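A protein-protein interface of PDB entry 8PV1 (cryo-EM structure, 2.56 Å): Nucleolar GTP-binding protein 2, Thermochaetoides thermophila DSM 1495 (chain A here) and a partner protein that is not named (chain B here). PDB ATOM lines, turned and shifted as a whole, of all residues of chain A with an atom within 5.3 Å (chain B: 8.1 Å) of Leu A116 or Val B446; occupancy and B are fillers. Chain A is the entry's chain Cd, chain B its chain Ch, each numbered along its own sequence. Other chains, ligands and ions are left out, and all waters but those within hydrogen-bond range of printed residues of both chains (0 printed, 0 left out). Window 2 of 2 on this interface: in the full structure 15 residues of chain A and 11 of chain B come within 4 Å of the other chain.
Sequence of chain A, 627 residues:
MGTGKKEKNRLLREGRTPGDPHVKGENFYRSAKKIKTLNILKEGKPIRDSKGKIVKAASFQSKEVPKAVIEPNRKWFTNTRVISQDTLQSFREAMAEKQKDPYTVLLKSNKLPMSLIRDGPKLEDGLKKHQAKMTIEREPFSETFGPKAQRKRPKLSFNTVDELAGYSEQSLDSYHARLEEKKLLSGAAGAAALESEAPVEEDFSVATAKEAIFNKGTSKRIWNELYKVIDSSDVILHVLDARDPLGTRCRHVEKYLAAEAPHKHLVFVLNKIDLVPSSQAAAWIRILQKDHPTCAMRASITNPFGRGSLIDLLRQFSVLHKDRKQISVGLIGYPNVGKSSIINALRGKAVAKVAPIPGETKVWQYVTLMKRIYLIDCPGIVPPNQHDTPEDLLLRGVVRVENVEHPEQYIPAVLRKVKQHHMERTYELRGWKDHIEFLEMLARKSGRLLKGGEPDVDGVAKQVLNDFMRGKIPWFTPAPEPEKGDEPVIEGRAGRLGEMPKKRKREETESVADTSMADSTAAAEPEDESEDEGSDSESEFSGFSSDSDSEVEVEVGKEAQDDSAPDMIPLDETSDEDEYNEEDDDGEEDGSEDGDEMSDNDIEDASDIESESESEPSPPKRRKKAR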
ATOM      1  N   ILE A  83      19.043 -15.372  -9.450  1.00  0.00           N
ATOM      2  CA  ILE A  83      19.244 -13.964  -9.767  1.00  0.00           C
ATOM      3  C   ILE A  83      19.608 -13.232  -8.481  1.00  0.00           C
ATOM      4  O   ILE A  83      19.169 -13.611  -7.390  1.00  0.00           O
ATOM      5  CB  ILE A  83      17.997 -13.356 -10.458  1.00  0.00           C
ATOM      6  CG1 ILE A  83      18.312 -11.988 -11.065  1.00  0.00           C
ATOM      7  CG2 ILE A  83      16.804 -13.277  -9.513  1.00  0.00           C
ATOM      8  CD1 ILE A  83      17.243 -11.472 -11.989  1.00  0.00           C
ATOM      9  N   LEU A  88      18.348  -7.638 -10.052  1.00  0.00           N
ATOM     10  CA  LEU A  88      16.922  -7.335  -9.998  1.00  0.00           C
ATOM     11  C   LEU A  88      16.668  -5.833  -9.972  1.00  0.00           C
ATOM     12  O   LEU A  88      15.783  -5.337 -10.676  1.00  0.00           O
ATOM     13  CB  LEU A  88      16.290  -7.999  -8.776  1.00  0.00           C
ATOM     14  CG  LEU A  88      15.821  -9.442  -8.936  1.00  0.00           C
ATOM     15  CD1 LEU A  88      15.464 -10.035  -7.587  1.00  0.00           C
ATOM     16  CD2 LEU A  88      14.638  -9.506  -9.880  1.00  0.00           C
ATOM     17  N   ARG A  92      14.713  -3.556 -12.720  1.00  0.00           N
ATOM     18  CA  ARG A  92      13.616  -2.669 -12.338  1.00  0.00           C
ATOM     19  C   ARG A  92      13.851  -1.251 -12.842  1.00  0.00           C
ATOM     20  O   ARG A  92      12.927  -0.607 -13.357  1.00  0.00           O
ATOM     21  CB  ARG A  92      13.433  -2.670 -10.821  1.00  0.00           C
ATOM     22  CG  ARG A  92      12.929  -3.978 -10.250  1.00  0.00           C
ATOM     23  CD  ARG A  92      12.498  -3.814  -8.810  1.00  0.00           C
ATOM     24  NE  ARG A  92      12.358  -5.097  -8.135  1.00  0.00           N
ATOM     25  CZ  ARG A  92      13.216  -5.568  -7.243  1.00  0.00           C
ATOM     26  NH1 ARG A  92      14.290  -4.883  -6.890  1.00  0.00           N
ATOM     27  NH2 ARG A  92      12.991  -6.756  -6.689  1.00  0.00           N
ATOM     28  N   PRO A 113      12.504 -13.401 -14.409  1.00  0.00           N
ATOM     29  CA  PRO A 113      11.386 -13.472 -13.447  1.00  0.00           C
ATOM     30  C   PRO A 113      10.608 -12.159 -13.421  1.00  0.00           C
ATOM     31  O   PRO A 113      10.836 -11.261 -12.612  1.00  0.00           O
ATOM     32  CB  PRO A 113      12.099 -13.760 -12.125  1.00  0.00           C
ATOM     33  CG  PRO A 113      13.442 -13.145 -12.284  1.00  0.00           C
ATOM     34  CD  PRO A 113      13.807 -13.274 -13.732  1.00  0.00           C
ATOM     35  N   MET A 114       9.653 -12.047 -14.348  1.00  0.00           N
ATOM     36  CA  MET A 114       8.983 -10.771 -14.583  1.00  0.00           C
ATOM     37  C   MET A 114       8.089 -10.365 -13.419  1.00  0.00           C
ATOM     38  O   MET A 114       7.801  -9.175 -13.250  1.00  0.00           O
ATOM     39  CB  MET A 114       8.168 -10.842 -15.876  1.00  0.00           C
ATOM     40  CG  MET A 114       8.988 -10.983 -17.160  1.00  0.00           C
ATOM     41  SD  MET A 114      10.401  -9.877 -17.414  1.00  0.00           S
ATOM     42  CE  MET A 114       9.721  -8.256 -17.057  1.00  0.00           C
ATOM     43  N   SER A 115       7.659 -11.322 -12.595  1.00  0.00           N
ATOM     44  CA  SER A 115       6.841 -10.984 -11.437  1.00  0.00           C
ATOM     45  C   SER A 115       7.631 -10.240 -10.368  1.00  0.00           C
ATOM     46  O   SER A 115       7.032  -9.537  -9.548  1.00  0.00           O
ATOM     47  CB  SER A 115       6.219 -12.249 -10.843  1.00  0.00           C
ATOM     48  OG  SER A 115       7.215 -13.144 -10.384  1.00  0.00           O
ATOM     49  N   LEU A 116       8.956 -10.375 -10.356  1.00  0.00           N
ATOM     50  CA  LEU A 116       9.805  -9.647  -9.423  1.00  0.00           C
ATOM     51  C   LEU A 116      10.346  -8.348  -9.998  1.00  0.00           C
ATOM     52  O   LEU A 116      10.963  -7.572  -9.263  1.00  0.00           O
ATOM     53  CB  LEU A 116      10.975 -10.526  -8.975  1.00  0.00           C
ATOM     54  CG  LEU A 116      10.640 -11.901  -8.401  1.00  0.00           C
ATOM     55  CD1 LEU A 116      11.908 -12.719  -8.249  1.00  0.00           C
ATOM     56  CD2 LEU A 116       9.921 -11.765  -7.072  1.00  0.00           C
ATOM     57  N   ILE A 117      10.136  -8.089 -11.290  1.00  0.00           N
ATOM     58  CA  ILE A 117      10.706  -6.932 -11.963  1.00  0.00           C
ATOM     59  C   ILE A 117       9.638  -5.920 -12.356  1.00  0.00           C
ATOM     60  O   ILE A 117       9.863  -4.707 -12.265  1.00  0.00           O
ATOM     61  CB  ILE A 117      11.529  -7.362 -13.196  1.00  0.00           C
ATOM     62  CG1 ILE A 117      12.520  -8.458 -12.815  1.00  0.00           C
ATOM     63  CG2 ILE A 117      12.311  -6.201 -13.741  1.00  0.00           C
ATOM     64  CD1 ILE A 117      13.199  -9.108 -13.996  1.00  0.00           C
ATOM     65  N   ARG A 118       8.472  -6.393 -12.795  1.00  0.00           N
ATOM     66  CA  ARG A 118       7.365  -5.499 -13.109  1.00  0.00           C
ATOM     67  C   ARG A 118       6.887  -4.783 -11.854  1.00  0.00           C
ATOM     68  O   ARG A 118       6.828  -5.361 -10.765  1.00  0.00           O
ATOM     69  CB  ARG A 118       6.201  -6.277 -13.723  1.00  0.00           C
ATOM     70  CG  ARG A 118       6.464  -6.845 -15.101  1.00  0.00           C
ATOM     71  CD  ARG A 118       5.226  -7.531 -15.651  1.00  0.00           C
ATOM     72  NE  ARG A 118       4.913  -8.754 -14.921  1.00  0.00           N
ATOM     73  CZ  ARG A 118       3.840  -8.918 -14.160  1.00  0.00           C
ATOM     74  NH1 ARG A 118       2.948  -7.953 -14.005  1.00  0.00           N
ATOM     75  NH2 ARG A 118       3.658 -10.079 -13.538  1.00  0.00           N
ATOM     76  N   TRP B 424       2.392  -7.893   4.042  1.00  0.00           N
ATOM     77  CA  TRP B 424       2.346  -9.214   3.432  1.00  0.00           C
ATOM     78  C   TRP B 424       2.468  -9.157   1.917  1.00  0.00           C
ATOM     79  O   TRP B 424       2.466 -10.208   1.268  1.00  0.00           O
ATOM     80  CB  TRP B 424       1.053  -9.938   3.819  1.00  0.00           C
ATOM     81  CG  TRP B 424       0.992 -10.397   5.249  1.00  0.00           C
ATOM     82  CD1 TRP B 424       1.174  -9.637   6.366  1.00  0.00           C
ATOM     83  CD2 TRP B 424       0.713 -11.722   5.711  1.00  0.00           C
ATOM     84  NE1 TRP B 424       1.032 -10.406   7.493  1.00  0.00           N
ATOM     85  CE2 TRP B 424       0.749 -11.691   7.117  1.00  0.00           C
ATOM     86  CE3 TRP B 424       0.439 -12.933   5.070  1.00  0.00           C
ATOM     87  CZ2 TRP B 424       0.521 -12.823   7.893  1.00  0.00           C
ATOM     88  CZ3 TRP B 424       0.214 -14.055   5.843  1.00  0.00           C
ATOM     89  CH2 TRP B 424       0.257 -13.992   7.239  1.00  0.00           C
ATOM     90  N   ASP B 425       2.575  -7.957   1.346  1.00  0.00           N
ATOM     91  CA  ASP B 425       2.845  -7.768  -0.071  1.00  0.00           C
ATOM     92  C   ASP B 425       4.339  -7.693  -0.361  1.00  0.00           C
ATOM     93  O   ASP B 425       4.744  -7.036  -1.325  1.00  0.00           O
ATOM     94  CB  ASP B 425       2.143  -6.509  -0.581  1.00  0.00           C
ATOM     95  CG  ASP B 425       2.438  -5.287   0.269  1.00  0.00           C
ATOM     96  OD1 ASP B 425       3.016  -5.444   1.364  1.00  0.00           O
ATOM     97  OD2 ASP B 425       2.097  -4.167  -0.160  1.00  0.00           O
ATOM     98  N   ASN B 426       5.155  -8.333   0.482  1.00  0.00           N
ATOM     99  CA  ASN B 426       6.606  -8.448   0.358  1.00  0.00           C
ATOM    100  C   ASN B 426       7.310  -7.099   0.405  1.00  0.00           C
ATOM    101  O   ASN B 426       8.396  -6.951  -0.163  1.00  0.00           O
ATOM    102  CB  ASN B 426       7.012  -9.188  -0.925  1.00  0.00           C
ATOM    103  CG  ASN B 426       6.201 -10.443  -1.159  1.00  0.00           C
ATOM    104  OD1 ASN B 426       5.710 -11.064  -0.223  1.00  0.00           O
ATOM    105  ND2 ASN B 426       6.078 -10.836  -2.419  1.00  0.00           N
ATOM    106  N   SER B 427       6.729  -6.102   1.070  1.00  0.00           N
ATOM    107  CA  SER B 427       7.235  -4.742   0.985  1.00  0.00           C
ATOM    108  C   SER B 427       7.283  -4.072   2.350  1.00  0.00           C
ATOM    109  O   SER B 427       6.432  -4.289   3.220  1.00  0.00           O
ATOM    110  CB  SER B 427       6.387  -3.894   0.029  1.00  0.00           C
ATOM    111  OG  SER B 427       5.158  -3.528   0.629  1.00  0.00           O
ATOM    112  N   ARG B 443      11.829  -2.363  -1.671  1.00  0.00           N
ATOM    113  CA  ARG B 443      11.484  -3.568  -2.410  1.00  0.00           C
ATOM    114  C   ARG B 443      12.695  -4.490  -2.472  1.00  0.00           C
ATOM    115  O   ARG B 443      13.833  -4.020  -2.552  1.00  0.00           O
ATOM    116  CB  ARG B 443      11.007  -3.202  -3.817  1.00  0.00           C
ATOM    117  CG  ARG B 443      10.348  -4.322  -4.595  1.00  0.00           C
ATOM    118  CD  ARG B 443       9.963  -3.845  -5.982  1.00  0.00           C
ATOM    119  NE  ARG B 443       9.299  -4.883  -6.761  1.00  0.00           N
ATOM    120  CZ  ARG B 443       8.919  -4.741  -8.023  1.00  0.00           C
ATOM    121  NH1 ARG B 443       9.113  -3.609  -8.680  1.00  0.00           N
ATOM    122  NH2 ARG B 443       8.326  -5.758  -8.640  1.00  0.00           N
ATOM    123  N   GLY B 444      12.445  -5.799  -2.469  1.00  0.00           N
ATOM    124  CA  GLY B 444      13.524  -6.767  -2.455  1.00  0.00           C
ATOM    125  C   GLY B 444      13.232  -8.051  -1.703  1.00  0.00           C
ATOM    126  O   GLY B 444      13.837  -9.084  -1.998  1.00  0.00           O
ATOM    127  N   HIS B 445      12.320  -8.015  -0.737  1.00  0.00           N
ATOM    128  CA  HIS B 445      11.827  -9.255  -0.154  1.00  0.00           C
ATOM    129  C   HIS B 445      10.902  -9.967  -1.135  1.00  0.00           C
ATOM    130  O   HIS B 445      10.200  -9.337  -1.930  1.00  0.00           O
ATOM    131  CB  HIS B 445      11.091  -8.987   1.156  1.00  0.00           C
ATOM    132  CG  HIS B 445      11.992  -8.812   2.337  1.00  0.00           C
ATOM    133  ND1 HIS B 445      12.872  -9.787   2.751  1.00  0.00           N
ATOM    134  CD2 HIS B 445      12.140  -7.782   3.204  1.00  0.00           C
ATOM    135  CE1 HIS B 445      13.523  -9.366   3.820  1.00  0.00           C
ATOM    136  NE2 HIS B 445      13.099  -8.152   4.115  1.00  0.00           N
ATOM    137  N   VAL B 446      10.902 -11.296  -1.072  1.00  0.00           N
ATOM    138  CA  VAL B 446      10.127 -12.124  -1.986  1.00  0.00           C
ATOM    139  C   VAL B 446       9.057 -12.937  -1.277  1.00  0.00           C
ATOM    140  O   VAL B 446       8.300 -13.653  -1.939  1.00  0.00           O
ATOM    141  CB  VAL B 446      11.042 -13.048  -2.815  1.00  0.00           C
ATOM    142  CG1 VAL B 446      11.823 -12.238  -3.834  1.00  0.00           C
ATOM    143  CG2 VAL B 446      11.986 -13.813  -1.910  1.00  0.00           C
ATOM    144  N   ALA B 447       8.974 -12.853   0.044  1.00  0.00           N
ATOM    145  CA  ALA B 447       7.933 -13.479   0.848  1.00  0.00           C
ATOM    146  C   ALA B 447       7.462 -12.424   1.842  1.00  0.00           C
ATOM    147  O   ALA B 447       8.146 -11.405   1.992  1.00  0.00           O
ATOM    148  CB  ALA B 447       8.459 -14.738   1.542  1.00  0.00           C
ATOM    149  N   PRO B 448       6.272 -12.586   2.487  1.00  0.00           N
ATOM    150  CA  PRO B 448       5.778 -11.559   3.422  1.00  0.00           C
ATOM    151  C   PRO B 448       6.745 -11.151   4.524  1.00  0.00           C
ATOM    152  O   PRO B 448       7.376 -11.996   5.165  1.00  0.00           O
ATOM    153  CB  PRO B 448       4.535 -12.223   4.021  1.00  0.00           C
ATOM    154  CG  PRO B 448       4.014 -13.055   2.928  1.00  0.00           C
ATOM    155  CD  PRO B 448       5.191 -13.520   2.112  1.00  0.00           C
ATOM    156  N   VAL B 449       6.860  -9.846   4.741  1.00  0.00           N
ATOM    157  CA  VAL B 449       7.776  -9.281   5.722  1.00  0.00           C
ATOM    158  C   VAL B 449       7.070  -9.275   7.067  1.00  0.00           C
ATOM    159  O   VAL B 449       6.007  -8.664   7.216  1.00  0.00           O
ATOM    160  CB  VAL B 449       8.217  -7.864   5.324  1.00  0.00           C
ATOM    161  CG1 VAL B 449       9.318  -7.380   6.245  1.00  0.00           C
ATOM    162  CG2 VAL B 449       8.670  -7.842   3.882  1.00  0.00           C
ATOM    163  N   SER B 465      11.894 -11.335   7.286  1.00  0.00           N
ATOM    164  CA  SER B 465      10.771 -11.783   6.475  1.00  0.00           C
ATOM    165  C   SER B 465      10.617 -13.297   6.510  1.00  0.00           C
ATOM    166  O   SER B 465      11.386 -14.021   7.145  1.00  0.00           O
ATOM    167  CB  SER B 465      10.921 -11.311   5.026  1.00  0.00           C
ATOM    168  OG  SER B 465       9.990 -11.958   4.181  1.00  0.00           O
ATOM    169  N   LYS B 466       9.579 -13.758   5.808  1.00  0.00           N
ATOM    170  CA  LYS B 466       9.278 -15.173   5.655  1.00  0.00           C
ATOM    171  C   LYS B 466      10.221 -15.855   4.670  1.00  0.00           C
ATOM    172  O   LYS B 466      10.364 -17.082   4.711  1.00  0.00           O
ATOM    173  CB  LYS B 466       7.810 -15.313   5.226  1.00  0.00           C
ATOM    174  CG  LYS B 466       7.274 -16.723   5.051  1.00  0.00           C
ATOM    175  CD  LYS B 466       5.833 -16.703   4.590  1.00  0.00           C
ATOM    176  CE  LYS B 466       5.286 -18.108   4.447  1.00  0.00           C
ATOM    177  NZ  LYS B 466       3.906 -18.104   3.895  1.00  0.00           N
ATOM    178  N   ASP B 467      10.926 -15.088   3.837  1.00  0.00           N
ATOM    179  CA  ASP B 467      11.875 -15.639   2.877  1.00  0.00           C
ATOM    180  C   ASP B 467      13.212 -16.025   3.502  1.00  0.00           C
ATOM    181  O   ASP B 467      14.193 -16.170   2.765  1.00  0.00           O
ATOM    182  CB  ASP B 467      12.087 -14.657   1.712  1.00  0.00           C
ATOM    183  CG  ASP B 467      12.685 -13.315   2.138  1.00  0.00           C
ATOM    184  OD1 ASP B 467      12.988 -13.098   3.328  1.00  0.00           O
ATOM    185  OD2 ASP B 467      12.851 -12.455   1.249  1.00  0.00           O
ATOM    186  N   CYS B 468      13.265 -16.153   4.829  1.00  0.00           N
ATOM    187  CA  CYS B 468      14.376 -16.602   5.662  1.00  0.00           C
ATOM    188  C   CYS B 468      15.505 -15.581   5.702  1.00  0.00           C
ATOM    189  O   CYS B 468      16.634 -15.953   6.040  1.00  0.00           O
ATOM    190  CB  CYS B 468      14.948 -17.959   5.219  1.00  0.00           C
ATOM    191  SG  CYS B 468      13.696 -19.199   4.820  1.00  0.00           S
ATOM    192  N   THR B 469      15.254 -14.317   5.367  1.00  0.00           N
ATOM    193  CA  THR B 469      16.304 -13.316   5.300  1.00  0.00           C
ATOM    194  C   THR B 469      15.983 -12.102   6.163  1.00  0.00           C
ATOM    195  O   THR B 469      14.813 -11.766   6.426  1.00  0.00           O
ATOM    196  CB  THR B 469      16.555 -12.832   3.858  1.00  0.00           C
ATOM    197  OG1 THR B 469      15.486 -11.974   3.443  1.00  0.00           O
ATOM    198  CG2 THR B 469      16.693 -13.991   2.889  1.00  0.00           C
ATOM    199  N   LYS B 471      17.000  -7.961   5.992  1.00  0.00           N
ATOM    200  CA  LYS B 471      17.520  -6.941   5.096  1.00  0.00           C
ATOM    201  C   LYS B 471      17.633  -5.619   5.832  1.00  0.00           C
ATOM    202  O   LYS B 471      16.675  -5.167   6.461  1.00  0.00           O
ATOM    203  CB  LYS B 471      16.646  -6.778   3.847  1.00  0.00           C
ATOM    204  CG  LYS B 471      16.564  -8.019   2.983  1.00  0.00           C
ATOM    205  CD  LYS B 471      16.082  -7.702   1.586  1.00  0.00           C
ATOM    206  CE  LYS B 471      15.671  -8.966   0.864  1.00  0.00           C
ATOM    207  NZ  LYS B 471      16.705 -10.024   0.982  1.00  0.00           N
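The guanidinium group of Arg A92 lies close to the guanidinium group of Arg B443. O of Arg A118 sits at hydrogen-bond distance from NH2 of Arg B443 (2.6 Å). The backbone carbonyl oxygen of Leu A116 lies within hydrogen-bond range of the guanidinium group of Arg B443 (3.3 Å).
NE of Arg A92 lies within hydrogen-bond range of O of Leu A116, at 3.1 Å. NE of Arg A118 sits close to O of Met A114, 3.4 Å away. N of Val B446 lies within hydrogen-bond range of OD2 of Asp B467, at 3.2 Å.
CD2 of Leu A116 touches CG1 of Val B446, 3.8 Å away. Arg B443 touches Ile A117 (NH1 to O, 3.8 Å).
Printed residues of chain B within 4 Å of Arg A92: Arg B443. Printed residues of chain B within 4 Å of Ile A117: Arg B443. Printed residues of chain B within 4 Å of Arg A118: Arg B443 (2.6 Å). Of the printed residues of chain A, Arg B443 touches Arg A92, Leu A116, Ile A117 and Arg A118. Of the printed residues of chain A, Val B446 touches Leu A116 (3.8 Å). Ala B447 touches none of the printed residues of chain A. Lys B471 touches none of the printed residues of chain A. The nearest residue of chain B that does not touch Leu A116 is His B445 (5.7 Å).
Of the 9 printed residues of chain A, 4 touch a printed residue of chain B. Printed residues of chain A that touch a printed residue of chain B: Arg A92, Leu A116, Ile A117 and Arg A118. Hydrophobic or aromatic side chains of chain A within 4 Å of the printed part of chain B: Leu A116. Printed residues of chain B that touch a printed residue of chain A: Arg B443 and Val B446. Among the printed residues, 5 pairs touch across the chains. Among the printed residues, no Asp or Glu carboxylate lies within 4 Å of a Lys or Arg side-chain nitrogen of the other chain.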
